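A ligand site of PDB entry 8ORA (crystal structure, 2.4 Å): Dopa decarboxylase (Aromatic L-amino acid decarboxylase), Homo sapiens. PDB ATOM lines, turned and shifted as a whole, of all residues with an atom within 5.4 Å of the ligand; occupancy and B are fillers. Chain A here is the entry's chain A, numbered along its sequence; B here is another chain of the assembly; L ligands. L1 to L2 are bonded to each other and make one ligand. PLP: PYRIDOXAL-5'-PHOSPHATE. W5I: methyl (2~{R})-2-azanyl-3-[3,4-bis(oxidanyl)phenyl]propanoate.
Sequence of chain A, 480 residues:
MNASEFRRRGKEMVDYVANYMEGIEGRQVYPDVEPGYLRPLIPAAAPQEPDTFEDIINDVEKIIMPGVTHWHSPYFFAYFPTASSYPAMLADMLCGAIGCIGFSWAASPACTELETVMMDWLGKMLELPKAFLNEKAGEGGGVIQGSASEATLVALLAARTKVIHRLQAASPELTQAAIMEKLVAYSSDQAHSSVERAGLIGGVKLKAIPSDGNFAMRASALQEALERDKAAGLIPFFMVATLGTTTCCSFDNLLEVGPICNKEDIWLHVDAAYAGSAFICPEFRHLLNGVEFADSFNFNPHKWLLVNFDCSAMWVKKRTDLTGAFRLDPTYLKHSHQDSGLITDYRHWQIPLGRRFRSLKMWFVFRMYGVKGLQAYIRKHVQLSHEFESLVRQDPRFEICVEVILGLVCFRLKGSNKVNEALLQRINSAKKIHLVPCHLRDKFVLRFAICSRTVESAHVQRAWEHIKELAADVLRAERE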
ATOM      1  N   TRP A  71      -6.813 -15.853  18.858  1.00  0.00           N
ATOM      2  CA  TRP A  71      -7.580 -14.850  18.133  1.00  0.00           C
ATOM      3  C   TRP A  71      -9.029 -15.255  17.967  1.00  0.00           C
ATOM      4  O   TRP A  71      -9.900 -14.398  17.798  1.00  0.00           O
ATOM      5  CB  TRP A  71      -6.950 -14.594  16.751  1.00  0.00           C
ATOM      6  CG  TRP A  71      -5.796 -13.651  16.766  1.00  0.00           C
ATOM      7  CD1 TRP A  71      -4.589 -13.840  17.382  1.00  0.00           C
ATOM      8  CD2 TRP A  71      -5.716 -12.376  16.117  1.00  0.00           C
ATOM      9  NE1 TRP A  71      -3.771 -12.754  17.153  1.00  0.00           N
ATOM     10  CE2 TRP A  71      -4.445 -11.840  16.378  1.00  0.00           C
ATOM     11  CE3 TRP A  71      -6.617 -11.632  15.342  1.00  0.00           C
ATOM     12  CZ2 TRP A  71      -4.039 -10.606  15.899  1.00  0.00           C
ATOM     13  CZ3 TRP A  71      -6.211 -10.405  14.857  1.00  0.00           C
ATOM     14  CH2 TRP A  71      -4.938  -9.901  15.138  1.00  0.00           C
ATOM     15  N   TYR A  79      -7.711  -5.689  18.488  1.00  0.00           N
ATOM     16  CA  TYR A  79      -7.416  -5.288  17.124  1.00  0.00           C
ATOM     17  C   TYR A  79      -8.644  -5.352  16.233  1.00  0.00           C
ATOM     18  O   TYR A  79      -9.616  -4.627  16.436  1.00  0.00           O
ATOM     19  CB  TYR A  79      -6.307  -6.159  16.537  1.00  0.00           C
ATOM     20  CG  TYR A  79      -5.140  -6.421  17.470  1.00  0.00           C
ATOM     21  CD1 TYR A  79      -4.236  -5.418  17.785  1.00  0.00           C
ATOM     22  CD2 TYR A  79      -4.955  -7.678  18.034  1.00  0.00           C
ATOM     23  CE1 TYR A  79      -3.172  -5.656  18.629  1.00  0.00           C
ATOM     24  CE2 TYR A  79      -3.896  -7.921  18.884  1.00  0.00           C
ATOM     25  CZ  TYR A  79      -3.004  -6.914  19.179  1.00  0.00           C
ATOM     26  OH  TYR A  79      -1.954  -7.154  20.026  1.00  0.00           O
ATOM     27  N   PHE A  80      -8.599  -6.217  15.228  1.00  0.00           N
ATOM     28  CA  PHE A  80      -9.692  -6.491  14.322  1.00  0.00           C
ATOM     29  C   PHE A  80      -9.778  -7.997  14.131  1.00  0.00           C
ATOM     30  O   PHE A  80      -8.795  -8.708  14.359  1.00  0.00           O
ATOM     31  CB  PHE A  80      -9.496  -5.787  12.972  1.00  0.00           C
ATOM     32  CG  PHE A  80     -10.059  -4.396  12.931  1.00  0.00           C
ATOM     33  CD1 PHE A  80     -11.254  -4.090  13.564  1.00  0.00           C
ATOM     34  CD2 PHE A  80      -9.384  -3.379  12.260  1.00  0.00           C
ATOM     35  CE1 PHE A  80     -11.768  -2.809  13.528  1.00  0.00           C
ATOM     36  CE2 PHE A  80      -9.898  -2.098  12.224  1.00  0.00           C
ATOM     37  CZ  PHE A  80     -11.090  -1.809  12.862  1.00  0.00           C
ATOM     38  N   PRO A  81     -10.937  -8.516  13.712  1.00  0.00           N
ATOM     39  CA  PRO A  81     -11.056  -9.964  13.515  1.00  0.00           C
ATOM     40  C   PRO A  81     -10.108 -10.465  12.434  1.00  0.00           C
ATOM     41  O   PRO A  81      -9.757  -9.742  11.508  1.00  0.00           O
ATOM     42  CB  PRO A  81     -12.519 -10.146  13.103  1.00  0.00           C
ATOM     43  CG  PRO A  81     -12.950  -8.808  12.616  1.00  0.00           C
ATOM     44  CD  PRO A  81     -12.207  -7.824  13.461  1.00  0.00           C
ATOM     45  N   THR A  82      -9.701 -11.720  12.578  1.00  0.00           N
ATOM     46  CA  THR A  82      -9.001 -12.443  11.527  1.00  0.00           C
ATOM     47  C   THR A  82      -9.811 -13.679  11.162  1.00  0.00           C
ATOM     48  O   THR A  82     -10.547 -14.216  11.995  1.00  0.00           O
ATOM     49  CB  THR A  82      -7.568 -12.818  11.945  1.00  0.00           C
ATOM     50  OG1 THR A  82      -6.807 -13.187  10.771  1.00  0.00           O
ATOM     51  CG2 THR A  82      -7.565 -13.980  12.921  1.00  0.00           C
ATOM     52  N   GLY A 146      -0.885 -10.252  -0.647  1.00  0.00           N
ATOM     53  CA  GLY A 146      -0.563 -10.883   0.616  1.00  0.00           C
ATOM     54  C   GLY A 146      -1.079 -10.116   1.814  1.00  0.00           C
ATOM     55  O   GLY A 146      -1.371 -10.701   2.856  1.00  0.00           O
ATOM     56  N   SER A 147      -1.193  -8.792   1.696  1.00  0.00           N
ATOM     57  CA  SER A 147      -1.635  -7.963   2.806  1.00  0.00           C
ATOM     58  C   SER A 147      -2.140  -6.635   2.269  1.00  0.00           C
ATOM     59  O   SER A 147      -1.826  -6.248   1.136  1.00  0.00           O
ATOM     60  CB  SER A 147      -0.513  -7.737   3.815  1.00  0.00           C
ATOM     61  OG  SER A 147       0.459  -6.842   3.285  1.00  0.00           O
ATOM     62  N   ALA A 148      -2.933  -5.946   3.082  1.00  0.00           N
ATOM     63  CA  ALA A 148      -3.353  -4.597   2.735  1.00  0.00           C
ATOM     64  C   ALA A 148      -2.175  -3.633   2.740  1.00  0.00           C
ATOM     65  O   ALA A 148      -2.170  -2.655   1.979  1.00  0.00           O
ATOM     66  CB  ALA A 148      -4.440  -4.111   3.696  1.00  0.00           C
ATOM     67  N   SER A 149      -1.174  -3.885   3.585  1.00  0.00           N
ATOM     68  CA  SER A 149       0.033  -3.054   3.592  1.00  0.00           C
ATOM     69  C   SER A 149       0.785  -3.185   2.279  1.00  0.00           C
ATOM     70  O   SER A 149       1.303  -2.199   1.752  1.00  0.00           O
ATOM     71  CB  SER A 149       0.926  -3.451   4.762  1.00  0.00           C
ATOM     72  OG  SER A 149       0.209  -3.425   5.983  1.00  0.00           O
ATOM     73  N   GLU A 150       0.842  -4.400   1.731  1.00  0.00           N
ATOM     74  CA  GLU A 150       1.483  -4.603   0.424  1.00  0.00           C
ATOM     75  C   GLU A 150       0.670  -3.955  -0.685  1.00  0.00           C
ATOM     76  O   GLU A 150       1.248  -3.373  -1.617  1.00  0.00           O
ATOM     77  CB  GLU A 150       1.674  -6.095   0.169  1.00  0.00           C
ATOM     78  CG  GLU A 150       2.766  -6.745   0.988  1.00  0.00           C
ATOM     79  CD  GLU A 150       2.660  -8.250   1.027  1.00  0.00           C
ATOM     80  OE1 GLU A 150       1.970  -8.774   1.922  1.00  0.00           O
ATOM     81  OE2 GLU A 150       3.269  -8.914   0.154  1.00  0.00           O
ATOM     82  N   HIS A 192      -3.683   3.853   8.934  1.00  0.00           N
ATOM     83  CA  HIS A 192      -2.860   2.766   9.433  1.00  0.00           C
ATOM     84  C   HIS A 192      -1.379   3.058   9.193  1.00  0.00           C
ATOM     85  O   HIS A 192      -1.014   3.851   8.322  1.00  0.00           O
ATOM     86  CB  HIS A 192      -3.255   1.444   8.766  1.00  0.00           C
ATOM     87  CG  HIS A 192      -2.604   0.234   9.364  1.00  0.00           C
ATOM     88  ND1 HIS A 192      -1.435  -0.302   8.879  1.00  0.00           N
ATOM     89  CD2 HIS A 192      -2.972  -0.557  10.401  1.00  0.00           C
ATOM     90  CE1 HIS A 192      -1.100  -1.359   9.592  1.00  0.00           C
ATOM     91  NE2 HIS A 192      -2.023  -1.535  10.527  1.00  0.00           N
ATOM     92  N   SER A 194       0.661   1.391   7.731  1.00  0.00           N
ATOM     93  CA  SER A 194       1.123   0.909   6.430  1.00  0.00           C
ATOM     94  C   SER A 194       1.326   2.052   5.443  1.00  0.00           C
ATOM     95  O   SER A 194       2.171   1.941   4.538  1.00  0.00           O
ATOM     96  CB  SER A 194       0.136  -0.108   5.871  1.00  0.00           C
ATOM     97  OG  SER A 194      -1.196   0.360   5.960  1.00  0.00           O
ATOM     98  N   THR A 242      -9.126   6.137   3.893  1.00  0.00           N
ATOM     99  CA  THR A 242      -9.371   4.971   4.721  1.00  0.00           C
ATOM    100  C   THR A 242     -10.858   4.848   5.041  1.00  0.00           C
ATOM    101  O   THR A 242     -11.479   5.803   5.512  1.00  0.00           O
ATOM    102  CB  THR A 242      -8.558   5.030   6.020  1.00  0.00           C
ATOM    103  OG1 THR A 242      -7.162   5.126   5.700  1.00  0.00           O
ATOM    104  CG2 THR A 242      -8.803   3.788   6.860  1.00  0.00           C
ATOM    105  N   LEU A 243     -11.419   3.669   4.793  1.00  0.00           N
ATOM    106  CA  LEU A 243     -12.772   3.321   5.192  1.00  0.00           C
ATOM    107  C   LEU A 243     -12.681   2.300   6.326  1.00  0.00           C
ATOM    108  O   LEU A 243     -12.129   1.223   6.138  1.00  0.00           O
ATOM    109  CB  LEU A 243     -13.579   2.760   4.019  1.00  0.00           C
ATOM    110  CG  LEU A 243     -13.792   3.691   2.821  1.00  0.00           C
ATOM    111  CD1 LEU A 243     -14.587   2.990   1.736  1.00  0.00           C
ATOM    112  CD2 LEU A 243     -14.495   4.973   3.263  1.00  0.00           C
ATOM    113  N   GLY A 244     -13.223   2.653   7.487  1.00  0.00           N
ATOM    114  CA  GLY A 244     -13.075   1.816   8.652  1.00  0.00           C
ATOM    115  C   GLY A 244     -11.682   1.912   9.227  1.00  0.00           C
ATOM    116  O   GLY A 244     -10.865   0.997   9.078  1.00  0.00           O
ATOM    117  N   THR A 245     -11.391   3.024   9.894  1.00  0.00           N
ATOM    118  CA  THR A 245     -10.061   3.265  10.422  1.00  0.00           C
ATOM    119  C   THR A 245      -9.716   2.275  11.534  1.00  0.00           C
ATOM    120  O   THR A 245     -10.593   1.784  12.252  1.00  0.00           O
ATOM    121  CB  THR A 245      -9.946   4.694  10.950  1.00  0.00           C
ATOM    122  OG1 THR A 245     -11.026   4.972  11.846  1.00  0.00           O
ATOM    123  CG2 THR A 245      -9.971   5.689   9.799  1.00  0.00           C
ATOM    124  N   THR A 246      -8.417   1.988  11.649  1.00  0.00           N
ATOM    125  CA  THR A 246      -7.939   1.114  12.718  1.00  0.00           C
ATOM    126  C   THR A 246      -8.290   1.667  14.090  1.00  0.00           C
ATOM    127  O   THR A 246      -8.620   0.898  15.008  1.00  0.00           O
ATOM    128  CB  THR A 246      -6.420   0.952  12.577  1.00  0.00           C
ATOM    129  OG1 THR A 246      -6.121   0.170  11.413  1.00  0.00           O
ATOM    130  CG2 THR A 246      -5.815   0.287  13.801  1.00  0.00           C
ATOM    131  N   ASP A 271      -8.315   2.337   1.271  1.00  0.00           N
ATOM    132  CA  ASP A 271      -7.964   1.283   2.211  1.00  0.00           C
ATOM    133  C   ASP A 271      -9.189   1.003   3.085  1.00  0.00           C
ATOM    134  O   ASP A 271      -9.519   1.802   3.968  1.00  0.00           O
ATOM    135  CB  ASP A 271      -6.759   1.688   3.056  1.00  0.00           C
ATOM    136  CG  ASP A 271      -6.309   0.597   4.026  1.00  0.00           C
ATOM    137  OD1 ASP A 271      -6.887  -0.522   3.999  1.00  0.00           O
ATOM    138  OD2 ASP A 271      -5.376   0.848   4.805  1.00  0.00           O
ATOM    139  N   ALA A 273      -9.687  -2.228   4.687  1.00  0.00           N
ATOM    140  CA  ALA A 273      -9.289  -3.584   5.026  1.00  0.00           C
ATOM    141  C   ALA A 273     -10.348  -4.300   5.855  1.00  0.00           C
ATOM    142  O   ALA A 273     -10.738  -5.432   5.550  1.00  0.00           O
ATOM    143  CB  ALA A 273      -7.958  -3.561   5.780  1.00  0.00           C
ATOM    144  N   TYR A 274     -10.845  -3.647   6.910  1.00  0.00           N
ATOM    145  CA  TYR A 274     -11.821  -4.273   7.787  1.00  0.00           C
ATOM    146  C   TYR A 274     -13.253  -4.042   7.323  1.00  0.00           C
ATOM    147  O   TYR A 274     -14.046  -4.988   7.249  1.00  0.00           O
ATOM    148  CB  TYR A 274     -11.644  -3.779   9.225  1.00  0.00           C
ATOM    149  CG  TYR A 274     -12.817  -4.079  10.122  1.00  0.00           C
ATOM    150  CD1 TYR A 274     -13.114  -5.379  10.507  1.00  0.00           C
ATOM    151  CD2 TYR A 274     -13.649  -3.058  10.578  1.00  0.00           C
ATOM    152  CE1 TYR A 274     -14.192  -5.656  11.314  1.00  0.00           C
ATOM    153  CE2 TYR A 274     -14.727  -3.327  11.392  1.00  0.00           C
ATOM    154  CZ  TYR A 274     -14.997  -4.631  11.765  1.00  0.00           C
ATOM    155  OH  TYR A 274     -16.075  -4.907  12.572  1.00  0.00           O
ATOM    156  N   ASN A 300      -9.542  -6.515   3.070  1.00  0.00           N
ATOM    157  CA  ASN A 300      -8.961  -7.782   3.489  1.00  0.00           C
ATOM    158  C   ASN A 300     -10.051  -8.800   3.763  1.00  0.00           C
ATOM    159  O   ASN A 300     -10.734  -8.719   4.797  1.00  0.00           O
ATOM    160  CB  ASN A 300      -8.099  -7.583   4.747  1.00  0.00           C
ATOM    161  CG  ASN A 300      -6.784  -6.894   4.442  1.00  0.00           C
ATOM    162  OD1 ASN A 300      -6.333  -6.863   3.294  1.00  0.00           O
ATOM    163  ND2 ASN A 300      -6.147  -6.360   5.477  1.00  0.00           N
ATOM    164  N   HIS A 302      -9.298 -11.653   4.700  1.00  0.00           N
ATOM    165  CA  HIS A 302      -8.731 -12.379   5.827  1.00  0.00           C
ATOM    166  C   HIS A 302      -8.997 -11.684   7.156  1.00  0.00           C
ATOM    167  O   HIS A 302      -8.433 -12.085   8.177  1.00  0.00           O
ATOM    168  CB  HIS A 302      -7.226 -12.611   5.630  1.00  0.00           C
ATOM    169  CG  HIS A 302      -6.408 -11.358   5.544  1.00  0.00           C
ATOM    170  ND1 HIS A 302      -5.451 -11.173   4.567  1.00  0.00           N
ATOM    171  CD2 HIS A 302      -6.381 -10.250   6.310  1.00  0.00           C
ATOM    172  CE1 HIS A 302      -4.877  -9.998   4.729  1.00  0.00           C
ATOM    173  NE2 HIS A 302      -5.430  -9.407   5.780  1.00  0.00           N
ATOM    174  N   LYS A 303      -9.847 -10.660   7.160  1.00  0.00           N
ATOM    175  CA  LYS A 303     -10.322 -10.030   8.381  1.00  0.00           C
ATOM    176  C   LYS A 303     -11.757 -10.422   8.693  1.00  0.00           C
ATOM    177  O   LYS A 303     -12.015 -11.074   9.705  1.00  0.00           O
ATOM    178  CB  LYS A 303     -10.220  -8.509   8.261  1.00  0.00           C
ATOM    179  CG  LYS A 303      -8.899  -7.916   8.640  1.00  0.00           C
ATOM    180  CD  LYS A 303      -8.969  -6.428   8.436  1.00  0.00           C
ATOM    181  CE  LYS A 303      -8.102  -5.710   9.424  1.00  0.00           C
ATOM    182  NZ  LYS A 303      -6.709  -6.224   9.343  1.00  0.00           N
ATOM    183  N   PHE A 309      -6.117 -15.996   6.404  1.00  0.00           N
ATOM    184  CA  PHE A 309      -4.876 -15.356   5.986  1.00  0.00           C
ATOM    185  C   PHE A 309      -3.965 -16.370   5.306  1.00  0.00           C
ATOM    186  O   PHE A 309      -3.802 -17.498   5.796  1.00  0.00           O
ATOM    187  CB  PHE A 309      -4.185 -14.735   7.212  1.00  0.00           C
ATOM    188  CG  PHE A 309      -3.035 -13.831   6.887  1.00  0.00           C
ATOM    189  CD1 PHE A 309      -1.742 -14.330   6.833  1.00  0.00           C
ATOM    190  CD2 PHE A 309      -3.236 -12.490   6.641  1.00  0.00           C
ATOM    191  CE1 PHE A 309      -0.668 -13.495   6.543  1.00  0.00           C
ATOM    192  CE2 PHE A 309      -2.171 -11.652   6.347  1.00  0.00           C
ATOM    193  CZ  PHE A 309      -0.891 -12.153   6.296  1.00  0.00           C
ATOM    194  N   ARG A 447     -10.773   0.104  22.991  1.00  0.00           N
ATOM    195  CA  ARG A 447     -11.475  -0.414  21.828  1.00  0.00           C
ATOM    196  C   ARG A 447     -12.076  -1.779  22.137  1.00  0.00           C
ATOM    197  O   ARG A 447     -11.438  -2.596  22.815  1.00  0.00           O
ATOM    198  CB  ARG A 447     -10.544  -0.530  20.620  1.00  0.00           C
ATOM    199  CG  ARG A 447      -9.700   0.696  20.350  1.00  0.00           C
ATOM    200  CD  ARG A 447      -8.564   0.389  19.380  1.00  0.00           C
ATOM    201  NE  ARG A 447      -9.042   0.065  18.036  1.00  0.00           N
ATOM    202  CZ  ARG A 447      -9.196  -1.160  17.562  1.00  0.00           C
ATOM    203  NH1 ARG A 447      -8.926  -2.229  18.305  1.00  0.00           N
ATOM    204  NH2 ARG A 447      -9.636  -1.332  16.317  1.00  0.00           N
ATOM    205  N   ILE B 101      -2.076 -13.868  13.890  1.00  0.00           N
ATOM    206  CA  ILE B 101      -1.474 -12.847  13.045  1.00  0.00           C
ATOM    207  C   ILE B 101      -0.335 -12.205  13.828  1.00  0.00           C
ATOM    208  O   ILE B 101      -0.518 -11.138  14.427  1.00  0.00           O
ATOM    209  CB  ILE B 101      -2.502 -11.810  12.574  1.00  0.00           C
ATOM    210  CG1 ILE B 101      -3.758 -12.512  12.031  1.00  0.00           C
ATOM    211  CG2 ILE B 101      -1.903 -10.896  11.515  1.00  0.00           C
ATOM    212  CD1 ILE B 101      -3.479 -13.438  10.865  1.00  0.00           C
ATOM    213  N   PHE B 103       2.077 -10.109  14.087  1.00  0.00           N
ATOM    214  CA  PHE B 103       2.836  -8.895  13.816  1.00  0.00           C
ATOM    215  C   PHE B 103       3.688  -8.496  15.008  1.00  0.00           C
ATOM    216  O   PHE B 103       4.754  -7.907  14.837  1.00  0.00           O
ATOM    217  CB  PHE B 103       1.894  -7.762  13.416  1.00  0.00           C
ATOM    218  CG  PHE B 103       0.598  -7.742  14.186  1.00  0.00           C
ATOM    219  CD1 PHE B 103       0.556  -7.347  15.509  1.00  0.00           C
ATOM    220  CD2 PHE B 103      -0.590  -8.115  13.565  1.00  0.00           C
ATOM    221  CE1 PHE B 103      -0.638  -7.329  16.203  1.00  0.00           C
ATOM    222  CE2 PHE B 103      -1.784  -8.105  14.252  1.00  0.00           C
ATOM    223  CZ  PHE B 103      -1.812  -7.707  15.573  1.00  0.00           C
ATOM    224  N   TYR B 332      -1.949   1.029  18.969  1.00  0.00           N
ATOM    225  CA  TYR B 332      -2.731  -0.187  18.796  1.00  0.00           C
ATOM    226  C   TYR B 332      -1.862  -1.402  18.506  1.00  0.00           C
ATOM    227  O   TYR B 332      -2.364  -2.527  18.563  1.00  0.00           O
ATOM    228  CB  TYR B 332      -3.766   0.000  17.687  1.00  0.00           C
ATOM    229  CG  TYR B 332      -3.242   0.609  16.402  1.00  0.00           C
ATOM    230  CD1 TYR B 332      -2.608  -0.172  15.450  1.00  0.00           C
ATOM    231  CD2 TYR B 332      -3.400   1.971  16.130  1.00  0.00           C
ATOM    232  CE1 TYR B 332      -2.132   0.372  14.270  1.00  0.00           C
ATOM    233  CE2 TYR B 332      -2.924   2.523  14.958  1.00  0.00           C
ATOM    234  CZ  TYR B 332      -2.297   1.714  14.022  1.00  0.00           C
ATOM    235  OH  TYR B 332      -1.825   2.260  12.856  1.00  0.00           O
ATOM    236  N   LEU B 333      -0.579  -1.209  18.212  1.00  0.00           N
ATOM    237  CA  LEU B 333       0.367  -2.310  18.003  1.00  0.00           C
ATOM    238  C   LEU B 333       1.463  -2.308  19.060  1.00  0.00           C
ATOM    239  O   LEU B 333       2.568  -2.819  18.821  1.00  0.00           O
ATOM    240  CB  LEU B 333       0.950  -2.240  16.594  1.00  0.00           C
ATOM    241  CG  LEU B 333      -0.081  -2.517  15.490  1.00  0.00           C
ATOM    242  CD1 LEU B 333       0.460  -2.264  14.098  1.00  0.00           C
ATOM    243  CD2 LEU B 333      -0.599  -3.938  15.617  1.00  0.00           C
ATOM    244  N   PRO B 352       5.210  -6.617   4.679  1.00  0.00           N
ATOM    245  CA  PRO B 352       3.881  -6.624   5.294  1.00  0.00           C
ATOM    246  C   PRO B 352       3.979  -6.410   6.799  1.00  0.00           C
ATOM    247  O   PRO B 352       5.052  -6.417   7.404  1.00  0.00           O
ATOM    248  CB  PRO B 352       3.337  -8.008   4.962  1.00  0.00           C
ATOM    249  CG  PRO B 352       4.554  -8.856   4.857  1.00  0.00           C
ATOM    250  CD  PRO B 352       5.588  -7.978   4.223  1.00  0.00           C
ATOM    251  N   LEU B 353       2.806  -6.227   7.407  1.00  0.00           N
ATOM    252  CA  LEU B 353       2.674  -6.197   8.852  1.00  0.00           C
ATOM    253  C   LEU B 353       2.237  -7.540   9.411  1.00  0.00           C
ATOM    254  O   LEU B 353       2.826  -8.042  10.366  1.00  0.00           O
ATOM    255  CB  LEU B 353       1.672  -5.111   9.278  1.00  0.00           C
ATOM    256  CG  LEU B 353       1.414  -5.032  10.789  1.00  0.00           C
ATOM    257  CD1 LEU B 353       2.411  -4.086  11.448  1.00  0.00           C
ATOM    258  CD2 LEU B 353      -0.021  -4.614  11.092  1.00  0.00           C
ATOM    259  N   GLY B 354       1.203  -8.139   8.823  1.00  0.00           N
ATOM    260  CA  GLY B 354       0.724  -9.422   9.266  1.00  0.00           C
ATOM    261  C   GLY B 354       1.588 -10.576   8.781  1.00  0.00           C
ATOM    262  O   GLY B 354       2.308 -10.481   7.788  1.00  0.00           O
HETATM  263  N1  PLP L   1      -5.363  -1.098   6.886  1.00  0.00           N
HETATM  264  C2  PLP L   1      -6.202  -0.996   7.926  1.00  0.00           C
HETATM  265  C2A PLP L   1      -7.220  -0.043   7.907  1.00  0.00           C
HETATM  266  C3  PLP L   1      -6.052  -1.850   9.019  1.00  0.00           C
HETATM  267  O3  PLP L   1      -6.913  -1.739  10.063  1.00  0.00           O
HETATM  268  C4  PLP L   1      -5.054  -2.810   9.076  1.00  0.00           C
HETATM  269  C4A PLP L   1      -4.949  -3.653  10.204  1.00  0.00           C
HETATM  270  C5  PLP L   1      -4.186  -2.916   7.995  1.00  0.00           C
HETATM  271  C6  PLP L   1      -4.345  -2.059   6.898  1.00  0.00           C
HETATM  272  C5A PLP L   1      -3.166  -3.862   7.990  1.00  0.00           C
HETATM  273  O4P PLP L   1      -3.311  -4.715   6.849  1.00  0.00           O
HETATM  274  P   PLP L   1      -2.595  -6.151   6.818  1.00  0.00           P
HETATM  275  O1P PLP L   1      -1.151  -5.794   6.224  1.00  0.00           O
HETATM  276  O2P PLP L   1      -3.316  -6.986   5.843  1.00  0.00           O
HETATM  277  O3P PLP L   1      -2.438  -6.627   8.223  1.00  0.00           O
HETATM  278  N1  W5I L   2      -5.765  -4.235  11.228  1.00  0.00           N
HETATM  279  C2  W5I L   2      -4.740  -6.845  11.971  1.00  0.00           C
HETATM  280  C3  W5I L   2      -3.906  -7.316  10.964  1.00  0.00           C
HETATM  281  C4  W5I L   2      -4.328  -8.424  10.231  1.00  0.00           C
HETATM  282  C5  W5I L   2      -5.544  -9.038  10.509  1.00  0.00           C
HETATM  283  C6  W5I L   2      -6.370  -8.569  11.519  1.00  0.00           C
HETATM  284  C7  W5I L   2      -4.388  -5.748  12.749  1.00  0.00           C
HETATM  285  C8  W5I L   2      -4.511  -4.417  12.006  1.00  0.00           C
HETATM  286  C9  W5I L   2      -4.170  -3.299  13.036  1.00  0.00           C
HETATM  287  C10 W5I L   2      -6.393  -3.125  14.121  1.00  0.00           C
HETATM  288  C1  W5I L   2      -5.956  -7.466  12.243  1.00  0.00           C
HETATM  289  O1  W5I L   2      -5.874 -10.120   9.745  1.00  0.00           O
HETATM  290  O2  W5I L   2      -3.583  -8.968   9.231  1.00  0.00           O
HETATM  291  O3  W5I L   2      -2.791  -3.343  13.389  1.00  0.00           O
HETATM  292  O4  W5I L   2      -4.977  -3.306  14.250  1.00  0.00           O
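The side-chain hydroxyl (OG1) of Thr 246 is in hydrogen-bond range of an oxygen (O3) of PLP L1, at 2.5 Å.
The backbone NH of Ser 149 is in hydrogen-bond range of an oxygen (O1P) of PLP L1 (3.3 Å).
The side-chain hydroxyl (OG) of Ser 149 sits at hydrogen-bond distance from an oxygen (O1P) of PLP L1 (2.7 Å).
N1 of PLP L1 lies within hydrogen-bond range of OD2 of Asp 271, 2.8 Å away.
The side-chain amino group of Lys 303 lies close to a nitrogen (N1) of W5I L2, 2.9 Å away.
An oxygen (O2P) of PLP L1 is in hydrogen-bond range of the side-chain amide nitrogen (ND2) of Asn 300, 2.9 Å away.
The backbone NH (N) of Ala 148 lies within hydrogen-bond range of an oxygen (O2P) of PLP L1 (3.0 Å).
NE2 of His 302 lies within hydrogen-bond range of O2P of PLP L1 (3.2 Å).
A ring nitrogen (NE2) of His 192 is in hydrogen-bond range of an oxygen (O3) of W5I L2 (3.5 Å).
OG1 of Thr 82 is in hydrogen-bond range of O1 of W5I L2.
The backbone NH (N) of Ser 149 sits close to the side-chain hydroxyl (OG) of Ser 147, 3.4 Å away.
The backbone NH (N) of Ala 273 is in hydrogen-bond range of the side-chain carboxylate (OD1) of Asp 271 (3.4 Å).
O of Asp 271 is in hydrogen-bond range of N of Leu 243 (2.8 Å).
The side-chain amide nitrogen (ND2) of Asn 300 lies within hydrogen-bond range of a ring nitrogen (NE2) of His 302, at 3.1 Å.
The backbone NH (N) of Asn 300 is in hydrogen-bond range of the backbone carbonyl oxygen (O) of Ala 273 (3.0 Å).
The side-chain hydroxyl of Ser 147 is in hydrogen-bond range of the side-chain carboxylate of Glu 150, at 2.8 Å.
O of His 302 sits at hydrogen-bond distance from OG1 of Thr 82.
N of Ser 194 sits at hydrogen-bond distance from ND1 of His 192.
Residues that only touch the ligand: Trp 71, Tyr 79, Phe 80, Pro 81, Ser 147, Gly 244, Ala 273, Ile 101 of chain B, Phe 103 of chain B, Tyr 332 of chain B, Leu 333 of chain B, Leu 353 of chain B and Gly 354 of chain B.
22 residues have an atom within 4 Å of the ligand: Trp 71, Tyr 79, Phe 80, Pro 81, Thr 82, Ser 147, Ala 148, Ser 149, His 192, Gly 244, Thr 246, Asp 271, Ala 273, Asn 300, His 302, Lys 303, Ile 101 of chain B, Phe 103 of chain B, Tyr 332 of chain B, Leu 333 of chain B, Leu 353 of chain B and Gly 354 of chain B.
The nearest printed residue that does not touch the ligand is Ser 194 (4.1 Å).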
